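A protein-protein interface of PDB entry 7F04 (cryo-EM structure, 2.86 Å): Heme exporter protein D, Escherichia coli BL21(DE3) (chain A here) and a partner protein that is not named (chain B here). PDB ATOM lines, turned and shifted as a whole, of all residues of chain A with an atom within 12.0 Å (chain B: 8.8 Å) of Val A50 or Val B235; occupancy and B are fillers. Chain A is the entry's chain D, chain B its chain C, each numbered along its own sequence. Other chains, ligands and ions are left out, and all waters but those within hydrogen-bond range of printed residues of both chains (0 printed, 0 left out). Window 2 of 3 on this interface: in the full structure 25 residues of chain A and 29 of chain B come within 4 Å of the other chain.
OH of Tyr B15 is in hydrogen-bond range of NE2 of His A43, at 3.3 Å.
CD2 of His A43 touches CD1 of Leu B226 (3.5 Å). Ile A46 touches Leu B226 (CG2 to CB, 3.5 Å). CD2 of Leu B227 touches CD1 of Ile A46 (3.6 Å). Val A50 touches Val B235 (CG1 to O, 3.3 Å).
Of the printed residues of chain A, Val B235 touches Val A50. No residue of chain B comes within 4 Å of Gly A49. No residue of chain B comes within 4 Å of Ala A51. Printed residues of chain A within 4 Å of Leu B226: His A43 and Ile A46. No residue of chain A comes within 4 Å of Glu B229. No residue of chain A comes within 4 Å of Pro B233. Trp B234 touches none of the printed residues of chain A. No residue of chain A comes within 4 Å of Ser B236. No residue of chain A comes within 4 Å of Glu B237. Of the printed residues of chain B, His A43 touches Tyr B15 and Leu B226. Of the printed residues of chain A, Tyr B15 touches His A43. Of the printed residues of chain A, Leu B227 touches Ile A46 (3.6 Å). Of the printed residues of chain B, Ile A46 touches Leu B226 (3.5 Å) and Leu B227 (3.6 Å). Gln A52 touches none of the printed residues of chain B. Arg A54 touches none of the printed residues of chain B. The nearest printed residue of chain B that does not touch Ile A46 is Lys B230 (6.1 Å).
Hydrophobic or aromatic side chains of chain A that line the printed part of chain B: His A43, Ile A46 and Val A50. Of the 15 printed residues of chain B, 4 touch a printed residue of chain A. Among the printed residues, 5 pairs touch across the chains.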
ATOM      1  N   MET A  41      -3.391   9.436  -3.459  1.00  0.00           N
ATOM      2  CA  MET A  41      -2.537   8.508  -2.731  1.00  0.00           C
ATOM      3  C   MET A  41      -3.341   7.643  -1.774  1.00  0.00           C
ATOM      4  O   MET A  41      -3.001   6.475  -1.572  1.00  0.00           O
ATOM      5  CB  MET A  41      -1.456   9.275  -1.972  1.00  0.00           C
ATOM      6  CG  MET A  41      -0.466  10.013  -2.863  1.00  0.00           C
ATOM      7  SD  MET A  41       0.524   8.930  -3.906  1.00  0.00           S
ATOM      8  CE  MET A  41       1.357  10.133  -4.938  1.00  0.00           C
ATOM      9  N   GLN A  42      -4.412   8.182  -1.190  1.00  0.00           N
ATOM     10  CA  GLN A  42      -5.255   7.383  -0.312  1.00  0.00           C
ATOM     11  C   GLN A  42      -6.037   6.344  -1.099  1.00  0.00           C
ATOM     12  O   GLN A  42      -6.224   5.219  -0.627  1.00  0.00           O
ATOM     13  CB  GLN A  42      -6.201   8.286   0.474  1.00  0.00           C
ATOM     14  CG  GLN A  42      -6.632   7.703   1.801  1.00  0.00           C
ATOM     15  CD  GLN A  42      -7.678   8.546   2.489  1.00  0.00           C
ATOM     16  OE1 GLN A  42      -8.263   9.445   1.886  1.00  0.00           O
ATOM     17  NE2 GLN A  42      -7.917   8.266   3.764  1.00  0.00           N
ATOM     18  N   HIS A  43      -6.505   6.696  -2.298  1.00  0.00           N
ATOM     19  CA  HIS A  43      -7.150   5.700  -3.146  1.00  0.00           C
ATOM     20  C   HIS A  43      -6.187   4.569  -3.477  1.00  0.00           C
ATOM     21  O   HIS A  43      -6.536   3.383  -3.385  1.00  0.00           O
ATOM     22  CB  HIS A  43      -7.665   6.356  -4.426  1.00  0.00           C
ATOM     23  CG  HIS A  43      -8.426   5.425  -5.317  1.00  0.00           C
ATOM     24  ND1 HIS A  43      -7.915   4.947  -6.502  1.00  0.00           N
ATOM     25  CD2 HIS A  43      -9.664   4.893  -5.198  1.00  0.00           C
ATOM     26  CE1 HIS A  43      -8.804   4.155  -7.074  1.00  0.00           C
ATOM     27  NE2 HIS A  43      -9.874   4.106  -6.303  1.00  0.00           N
ATOM     28  N   ARG A  44      -4.956   4.922  -3.852  1.00  0.00           N
ATOM     29  CA  ARG A  44      -3.966   3.901  -4.178  1.00  0.00           C
ATOM     30  C   ARG A  44      -3.633   3.044  -2.962  1.00  0.00           C
ATOM     31  O   ARG A  44      -3.499   1.821  -3.074  1.00  0.00           O
ATOM     32  CB  ARG A  44      -2.707   4.560  -4.740  1.00  0.00           C
ATOM     33  CG  ARG A  44      -2.849   5.035  -6.177  1.00  0.00           C
ATOM     34  CD  ARG A  44      -1.589   5.738  -6.655  1.00  0.00           C
ATOM     35  NE  ARG A  44      -1.216   5.334  -8.006  1.00  0.00           N
ATOM     36  CZ  ARG A  44      -0.583   4.208  -8.305  1.00  0.00           C
ATOM     37  NH1 ARG A  44      -0.231   3.342  -7.369  1.00  0.00           N
ATOM     38  NH2 ARG A  44      -0.295   3.944  -9.576  1.00  0.00           N
ATOM     39  N   ALA A  45      -3.498   3.666  -1.789  1.00  0.00           N
ATOM     40  CA  ALA A  45      -3.192   2.921  -0.574  1.00  0.00           C
ATOM     41  C   ALA A  45      -4.326   1.982  -0.195  1.00  0.00           C
ATOM     42  O   ALA A  45      -4.083   0.856   0.254  1.00  0.00           O
ATOM     43  CB  ALA A  45      -2.895   3.887   0.572  1.00  0.00           C
ATOM     44  N   ILE A  46      -5.571   2.433  -0.350  1.00  0.00           N
ATOM     45  CA  ILE A  46      -6.715   1.575  -0.064  1.00  0.00           C
ATOM     46  C   ILE A  46      -6.720   0.376  -0.998  1.00  0.00           C
ATOM     47  O   ILE A  46      -6.912  -0.766  -0.566  1.00  0.00           O
ATOM     48  CB  ILE A  46      -8.022   2.380  -0.175  1.00  0.00           C
ATOM     49  CG1 ILE A  46      -8.232   3.237   1.070  1.00  0.00           C
ATOM     50  CG2 ILE A  46      -9.200   1.450  -0.368  1.00  0.00           C
ATOM     51  CD1 ILE A  46      -9.023   4.497   0.801  1.00  0.00           C
ATOM     52  N   LEU A  47      -6.497   0.612  -2.294  1.00  0.00           N
ATOM     53  CA  LEU A  47      -6.463  -0.502  -3.237  1.00  0.00           C
ATOM     54  C   LEU A  47      -5.296  -1.440  -2.958  1.00  0.00           C
ATOM     55  O   LEU A  47      -5.387  -2.640  -3.234  1.00  0.00           O
ATOM     56  CB  LEU A  47      -6.395   0.018  -4.672  1.00  0.00           C
ATOM     57  CG  LEU A  47      -7.694   0.575  -5.253  1.00  0.00           C
ATOM     58  CD1 LEU A  47      -7.519   0.879  -6.728  1.00  0.00           C
ATOM     59  CD2 LEU A  47      -8.838  -0.394  -5.038  1.00  0.00           C
ATOM     60  N   ARG A  48      -4.189  -0.914  -2.426  1.00  0.00           N
ATOM     61  CA  ARG A  48      -3.085  -1.779  -2.018  1.00  0.00           C
ATOM     62  C   ARG A  48      -3.485  -2.670  -0.849  1.00  0.00           C
ATOM     63  O   ARG A  48      -3.175  -3.865  -0.839  1.00  0.00           O
ATOM     64  CB  ARG A  48      -1.861  -0.939  -1.651  1.00  0.00           C
ATOM     65  CG  ARG A  48      -1.112  -0.366  -2.842  1.00  0.00           C
ATOM     66  CD  ARG A  48      -0.468  -1.459  -3.673  1.00  0.00           C
ATOM     67  NE  ARG A  48       0.152  -0.930  -4.881  1.00  0.00           N
ATOM     68  CZ  ARG A  48       1.446  -0.671  -5.007  1.00  0.00           C
ATOM     69  NH1 ARG A  48       2.295  -0.894  -4.018  1.00  0.00           N
ATOM     70  NH2 ARG A  48       1.899  -0.178  -6.155  1.00  0.00           N
ATOM     71  N   GLY A  49      -4.179  -2.107   0.141  1.00  0.00           N
ATOM     72  CA  GLY A  49      -4.607  -2.900   1.279  1.00  0.00           C
ATOM     73  C   GLY A  49      -5.682  -3.910   0.935  1.00  0.00           C
ATOM     74  O   GLY A  49      -5.828  -4.923   1.625  1.00  0.00           O
ATOM     75  N   VAL A  50      -6.456  -3.649  -0.122  1.00  0.00           N
ATOM     76  CA  VAL A  50      -7.450  -4.619  -0.571  1.00  0.00           C
ATOM     77  C   VAL A  50      -6.764  -5.887  -1.061  1.00  0.00           C
ATOM     78  O   VAL A  50      -7.183  -7.004  -0.737  1.00  0.00           O
ATOM     79  CB  VAL A  50      -8.350  -4.001  -1.657  1.00  0.00           C
ATOM     80  CG1 VAL A  50      -9.128  -5.084  -2.388  1.00  0.00           C
ATOM     81  CG2 VAL A  50      -9.300  -2.988  -1.041  1.00  0.00           C
ATOM     82  N   ALA A  51      -5.698  -5.735  -1.849  1.00  0.00           N
ATOM     83  CA  ALA A  51      -4.894  -6.880  -2.251  1.00  0.00           C
ATOM     84  C   ALA A  51      -4.008  -7.394  -1.122  1.00  0.00           C
ATOM     85  O   ALA A  51      -3.672  -8.583  -1.110  1.00  0.00           O
ATOM     86  CB  ALA A  51      -4.033  -6.524  -3.464  1.00  0.00           C
ATOM     87  N   GLN A  52      -3.619  -6.528  -0.184  1.00  0.00           N
ATOM     88  CA  GLN A  52      -2.833  -6.982   0.959  1.00  0.00           C
ATOM     89  C   GLN A  52      -3.634  -7.938   1.833  1.00  0.00           C
ATOM     90  O   GLN A  52      -3.109  -8.963   2.284  1.00  0.00           O
ATOM     91  CB  GLN A  52      -2.353  -5.783   1.778  1.00  0.00           C
ATOM     92  CG  GLN A  52      -1.498  -6.154   2.980  1.00  0.00           C
ATOM     93  CD  GLN A  52      -2.296  -6.227   4.267  1.00  0.00           C
ATOM     94  OE1 GLN A  52      -3.237  -5.461   4.471  1.00  0.00           O
ATOM     95  NE2 GLN A  52      -1.925  -7.152   5.142  1.00  0.00           N
ATOM     96  N   GLN A  53      -4.906  -7.623   2.083  1.00  0.00           N
ATOM     97  CA  GLN A  53      -5.763  -8.520   2.847  1.00  0.00           C
ATOM     98  C   GLN A  53      -6.087  -9.800   2.092  1.00  0.00           C
ATOM     99  O   GLN A  53      -6.612 -10.739   2.697  1.00  0.00           O
ATOM    100  CB  GLN A  53      -7.056  -7.809   3.242  1.00  0.00           C
ATOM    101  CG  GLN A  53      -6.884  -6.806   4.367  1.00  0.00           C
ATOM    102  CD  GLN A  53      -6.524  -7.465   5.681  1.00  0.00           C
ATOM    103  OE1 GLN A  53      -6.879  -8.616   5.930  1.00  0.00           O
ATOM    104  NE2 GLN A  53      -5.810  -6.737   6.533  1.00  0.00           N
ATOM    105  N   ARG A  54      -5.796  -9.853   0.796  1.00  0.00           N
ATOM    106  CA  ARG A  54      -5.911 -11.083   0.015  1.00  0.00           C
ATOM    107  C   ARG A  54      -4.634 -11.912   0.121  1.00  0.00           C
ATOM    108  O   ARG A  54      -4.026 -12.306  -0.875  1.00  0.00           O
ATOM    109  CB  ARG A  54      -6.236 -10.742  -1.435  1.00  0.00           C
ATOM    110  CG  ARG A  54      -6.833 -11.888  -2.234  1.00  0.00           C
ATOM    111  CD  ARG A  54      -7.441 -11.389  -3.536  1.00  0.00           C
ATOM    112  NE  ARG A  54      -6.492 -10.611  -4.322  1.00  0.00           N
ATOM    113  CZ  ARG A  54      -5.600 -11.131  -5.154  1.00  0.00           C
ATOM    114  NH1 ARG A  54      -5.500 -12.439  -5.332  1.00  0.00           N
ATOM    115  NH2 ARG A  54      -4.787 -10.319  -5.824  1.00  0.00           N
ATOM    116  N   ALA A  55      -4.219 -12.172   1.358  1.00  0.00           N
ATOM    117  CA  ALA A  55      -3.000 -12.922   1.636  1.00  0.00           C
ATOM    118  C   ALA A  55      -3.017 -13.457   3.063  1.00  0.00           C
ATOM    119  O   ALA A  55      -2.748 -12.723   4.014  1.00  0.00           O
ATOM    120  CB  ALA A  55      -1.775 -12.050   1.412  1.00  0.00           C
ATOM    121  N   PRO B  12     -23.267  -0.426  -4.380  1.00  0.00           N
ATOM    122  CA  PRO B  12     -21.877  -0.013  -4.641  1.00  0.00           C
ATOM    123  C   PRO B  12     -21.603   0.396  -6.085  1.00  0.00           C
ATOM    124  O   PRO B  12     -20.451   0.646  -6.445  1.00  0.00           O
ATOM    125  CB  PRO B  12     -21.063  -1.259  -4.263  1.00  0.00           C
ATOM    126  CG  PRO B  12     -22.055  -2.375  -4.168  1.00  0.00           C
ATOM    127  CD  PRO B  12     -23.306  -1.725  -3.690  1.00  0.00           C
ATOM    128  N   TYR B  15     -19.790   3.765  -6.696  1.00  0.00           N
ATOM    129  CA  TYR B  15     -18.355   3.813  -6.959  1.00  0.00           C
ATOM    130  C   TYR B  15     -18.076   3.932  -8.450  1.00  0.00           C
ATOM    131  O   TYR B  15     -17.260   4.758  -8.874  1.00  0.00           O
ATOM    132  CB  TYR B  15     -17.694   2.563  -6.381  1.00  0.00           C
ATOM    133  CG  TYR B  15     -16.205   2.419  -6.628  1.00  0.00           C
ATOM    134  CD1 TYR B  15     -15.723   1.897  -7.823  1.00  0.00           C
ATOM    135  CD2 TYR B  15     -15.286   2.748  -5.647  1.00  0.00           C
ATOM    136  CE1 TYR B  15     -14.373   1.753  -8.046  1.00  0.00           C
ATOM    137  CE2 TYR B  15     -13.934   2.598  -5.862  1.00  0.00           C
ATOM    138  CZ  TYR B  15     -13.483   2.105  -7.062  1.00  0.00           C
ATOM    139  OH  TYR B  15     -12.133   1.957  -7.275  1.00  0.00           O
ATOM    140  N   ILE B 225     -16.264   5.108   0.082  1.00  0.00           N
ATOM    141  CA  ILE B 225     -16.984   3.897  -0.297  1.00  0.00           C
ATOM    142  C   ILE B 225     -16.073   2.686  -0.178  1.00  0.00           C
ATOM    143  O   ILE B 225     -16.474   1.633   0.334  1.00  0.00           O
ATOM    144  CB  ILE B 225     -17.552   4.039  -1.720  1.00  0.00           C
ATOM    145  CG1 ILE B 225     -18.810   4.903  -1.711  1.00  0.00           C
ATOM    146  CG2 ILE B 225     -17.848   2.676  -2.318  1.00  0.00           C
ATOM    147  CD1 ILE B 225     -19.159   5.462  -3.061  1.00  0.00           C
ATOM    148  N   LEU B 226     -14.834   2.810  -0.659  1.00  0.00           N
ATOM    149  CA  LEU B 226     -13.887   1.707  -0.515  1.00  0.00           C
ATOM    150  C   LEU B 226     -13.609   1.399   0.954  1.00  0.00           C
ATOM    151  O   LEU B 226     -13.603   0.231   1.360  1.00  0.00           O
ATOM    152  CB  LEU B 226     -12.587   2.028  -1.246  1.00  0.00           C
ATOM    153  CG  LEU B 226     -12.602   1.846  -2.761  1.00  0.00           C
ATOM    154  CD1 LEU B 226     -11.353   2.445  -3.375  1.00  0.00           C
ATOM    155  CD2 LEU B 226     -12.733   0.378  -3.123  1.00  0.00           C
ATOM    156  N   LEU B 227     -13.386   2.436   1.765  1.00  0.00           N
ATOM    157  CA  LEU B 227     -13.125   2.224   3.187  1.00  0.00           C
ATOM    158  C   LEU B 227     -14.288   1.522   3.872  1.00  0.00           C
ATOM    159  O   LEU B 227     -14.080   0.651   4.725  1.00  0.00           O
ATOM    160  CB  LEU B 227     -12.830   3.552   3.883  1.00  0.00           C
ATOM    161  CG  LEU B 227     -11.555   4.286   3.492  1.00  0.00           C
ATOM    162  CD1 LEU B 227     -11.497   5.640   4.166  1.00  0.00           C
ATOM    163  CD2 LEU B 227     -10.382   3.440   3.933  1.00  0.00           C
ATOM    164  N   MET B 228     -15.518   1.895   3.526  1.00  0.00           N
ATOM    165  CA  MET B 228     -16.676   1.246   4.129  1.00  0.00           C
ATOM    166  C   MET B 228     -16.774  -0.205   3.680  1.00  0.00           C
ATOM    167  O   MET B 228     -16.771  -1.125   4.505  1.00  0.00           O
ATOM    168  CB  MET B 228     -17.953   2.001   3.771  1.00  0.00           C
ATOM    169  CG  MET B 228     -19.188   1.408   4.417  1.00  0.00           C
ATOM    170  SD  MET B 228     -20.688   2.306   4.009  1.00  0.00           S
ATOM    171  CE  MET B 228     -20.861   1.810   2.299  1.00  0.00           C
ATOM    172  N   GLU B 229     -16.861  -0.431   2.373  1.00  0.00           N
ATOM    173  CA  GLU B 229     -16.992  -1.786   1.841  1.00  0.00           C
ATOM    174  C   GLU B 229     -15.638  -2.392   1.487  1.00  0.00           C
ATOM    175  O   GLU B 229     -15.457  -2.957   0.414  1.00  0.00           O
ATOM    176  CB  GLU B 229     -17.911  -1.773   0.627  1.00  0.00           C
ATOM    177  CG  GLU B 229     -19.281  -1.189   0.887  1.00  0.00           C
ATOM    178  CD  GLU B 229     -20.353  -1.862   0.061  1.00  0.00           C
ATOM    179  OE1 GLU B 229     -20.023  -2.380  -1.026  1.00  0.00           O
ATOM    180  OE2 GLU B 229     -21.524  -1.874   0.496  1.00  0.00           O
ATOM    181  N   LYS B 230     -14.675  -2.298   2.402  1.00  0.00           N
ATOM    182  CA  LYS B 230     -13.375  -2.923   2.189  1.00  0.00           C
ATOM    183  C   LYS B 230     -13.413  -4.442   2.307  1.00  0.00           C
ATOM    184  O   LYS B 230     -12.412  -5.091   1.983  1.00  0.00           O
ATOM    185  CB  LYS B 230     -12.357  -2.357   3.177  1.00  0.00           C
ATOM    186  CG  LYS B 230     -12.700  -2.606   4.631  1.00  0.00           C
ATOM    187  CD  LYS B 230     -11.502  -2.351   5.525  1.00  0.00           C
ATOM    188  CE  LYS B 230     -11.163  -0.871   5.583  1.00  0.00           C
ATOM    189  NZ  LYS B 230     -10.057  -0.594   6.538  1.00  0.00           N
ATOM    190  N   ARG B 231     -14.526  -5.025   2.757  1.00  0.00           N
ATOM    191  CA  ARG B 231     -14.614  -6.464   2.962  1.00  0.00           C
ATOM    192  C   ARG B 231     -15.603  -7.166   2.042  1.00  0.00           C
ATOM    193  O   ARG B 231     -15.600  -8.401   1.992  1.00  0.00           O
ATOM    194  CB  ARG B 231     -14.990  -6.772   4.419  1.00  0.00           C
ATOM    195  CG  ARG B 231     -13.878  -6.520   5.420  1.00  0.00           C
ATOM    196  CD  ARG B 231     -14.325  -6.872   6.829  1.00  0.00           C
ATOM    197  NE  ARG B 231     -13.273  -6.651   7.813  1.00  0.00           N
ATOM    198  CZ  ARG B 231     -13.399  -6.886   9.112  1.00  0.00           C
ATOM    199  NH1 ARG B 231     -14.527  -7.353   9.622  1.00  0.00           N
ATOM    200  NH2 ARG B 231     -12.370  -6.650   9.919  1.00  0.00           N
ATOM    201  N   ARG B 232     -16.442  -6.430   1.320  1.00  0.00           N
ATOM    202  CA  ARG B 232     -17.449  -7.064   0.484  1.00  0.00           C
ATOM    203  C   ARG B 232     -16.798  -7.756  -0.714  1.00  0.00           C
ATOM    204  O   ARG B 232     -15.733  -7.342  -1.178  1.00  0.00           O
ATOM    205  CB  ARG B 232     -18.475  -6.039   0.005  1.00  0.00           C
ATOM    206  CG  ARG B 232     -19.651  -5.846   0.954  1.00  0.00           C
ATOM    207  CD  ARG B 232     -19.231  -5.154   2.238  1.00  0.00           C
ATOM    208  NE  ARG B 232     -20.367  -4.839   3.094  1.00  0.00           N
ATOM    209  CZ  ARG B 232     -20.264  -4.327   4.313  1.00  0.00           C
ATOM    210  NH1 ARG B 232     -19.088  -4.054   4.852  1.00  0.00           N
ATOM    211  NH2 ARG B 232     -21.370  -4.081   5.009  1.00  0.00           N
ATOM    212  N   PRO B 233     -17.418  -8.824  -1.228  1.00  0.00           N
ATOM    213  CA  PRO B 233     -16.838  -9.521  -2.387  1.00  0.00           C
ATOM    214  C   PRO B 233     -16.801  -8.679  -3.647  1.00  0.00           C
ATOM    215  O   PRO B 233     -16.111  -9.055  -4.602  1.00  0.00           O
ATOM    216  CB  PRO B 233     -17.755 -10.739  -2.561  1.00  0.00           C
ATOM    217  CG  PRO B 233     -19.041 -10.335  -1.927  1.00  0.00           C
ATOM    218  CD  PRO B 233     -18.657  -9.469  -0.764  1.00  0.00           C
ATOM    219  N   TRP B 234     -17.529  -7.564  -3.686  1.00  0.00           N
ATOM    220  CA  TRP B 234     -17.512  -6.693  -4.855  1.00  0.00           C
ATOM    221  C   TRP B 234     -16.148  -6.057  -5.093  1.00  0.00           C
ATOM    222  O   TRP B 234     -15.877  -5.598  -6.208  1.00  0.00           O
ATOM    223  CB  TRP B 234     -18.559  -5.594  -4.697  1.00  0.00           C
ATOM    224  CG  TRP B 234     -18.607  -4.696  -5.866  1.00  0.00           C
ATOM    225  CD1 TRP B 234     -18.978  -5.019  -7.137  1.00  0.00           C
ATOM    226  CD2 TRP B 234     -18.176  -3.336  -5.906  1.00  0.00           C
ATOM    227  NE1 TRP B 234     -18.853  -3.925  -7.958  1.00  0.00           N
ATOM    228  CE2 TRP B 234     -18.356  -2.880  -7.225  1.00  0.00           C
ATOM    229  CE3 TRP B 234     -17.674  -2.451  -4.946  1.00  0.00           C
ATOM    230  CZ2 TRP B 234     -18.051  -1.580  -7.609  1.00  0.00           C
ATOM    231  CZ3 TRP B 234     -17.373  -1.167  -5.330  1.00  0.00           C
ATOM    232  CH2 TRP B 234     -17.562  -0.743  -6.651  1.00  0.00           C
ATOM    233  N   VAL B 235     -15.278  -6.041  -4.087  1.00  0.00           N
ATOM    234  CA  VAL B 235     -14.020  -5.306  -4.153  1.00  0.00           C
ATOM    235  C   VAL B 235     -12.931  -6.318  -4.501  1.00  0.00           C
ATOM    236  O   VAL B 235     -11.756  -6.154  -4.154  1.00  0.00           O
ATOM    237  CB  VAL B 235     -13.765  -4.558  -2.829  1.00  0.00           C
ATOM    238  CG1 VAL B 235     -12.518  -3.680  -2.891  1.00  0.00           C
ATOM    239  CG2 VAL B 235     -14.968  -3.722  -2.484  1.00  0.00           C
ATOM    240  N   SER B 236     -13.330  -7.388  -5.191  1.00  0.00           N
ATOM    241  CA  SER B 236     -12.376  -8.381  -5.669  1.00  0.00           C
ATOM    242  C   SER B 236     -11.331  -7.780  -6.597  1.00  0.00           C
ATOM    243  O   SER B 236     -10.265  -8.379  -6.781  1.00  0.00           O
ATOM    244  CB  SER B 236     -13.116  -9.506  -6.391  1.00  0.00           C
ATOM    245  OG  SER B 236     -13.741  -9.022  -7.568  1.00  0.00           O
ATOM    246  N   GLU B 237     -11.615  -6.626  -7.196  1.00  0.00           N
ATOM    247  CA  GLU B 237     -10.651  -5.919  -8.035  1.00  0.00           C
ATOM    248  C   GLU B 237      -9.392  -5.549  -7.252  1.00  0.00           C
ATOM    249  O   GLU B 237      -8.435  -6.320  -7.182  1.00  0.00           O
ATOM    250  CB  GLU B 237     -11.286  -4.658  -8.622  1.00  0.00           C
ATOM    251  CG  GLU B 237     -11.459  -3.536  -7.607  1.00  0.00           C
ATOM    252  CD  GLU B 237     -12.619  -2.617  -7.933  1.00  0.00           C
ATOM    253  OE1 GLU B 237     -12.942  -2.462  -9.129  1.00  0.00           O
ATOM    254  OE2 GLU B 237     -13.208  -2.047  -6.992  1.00  0.00           O
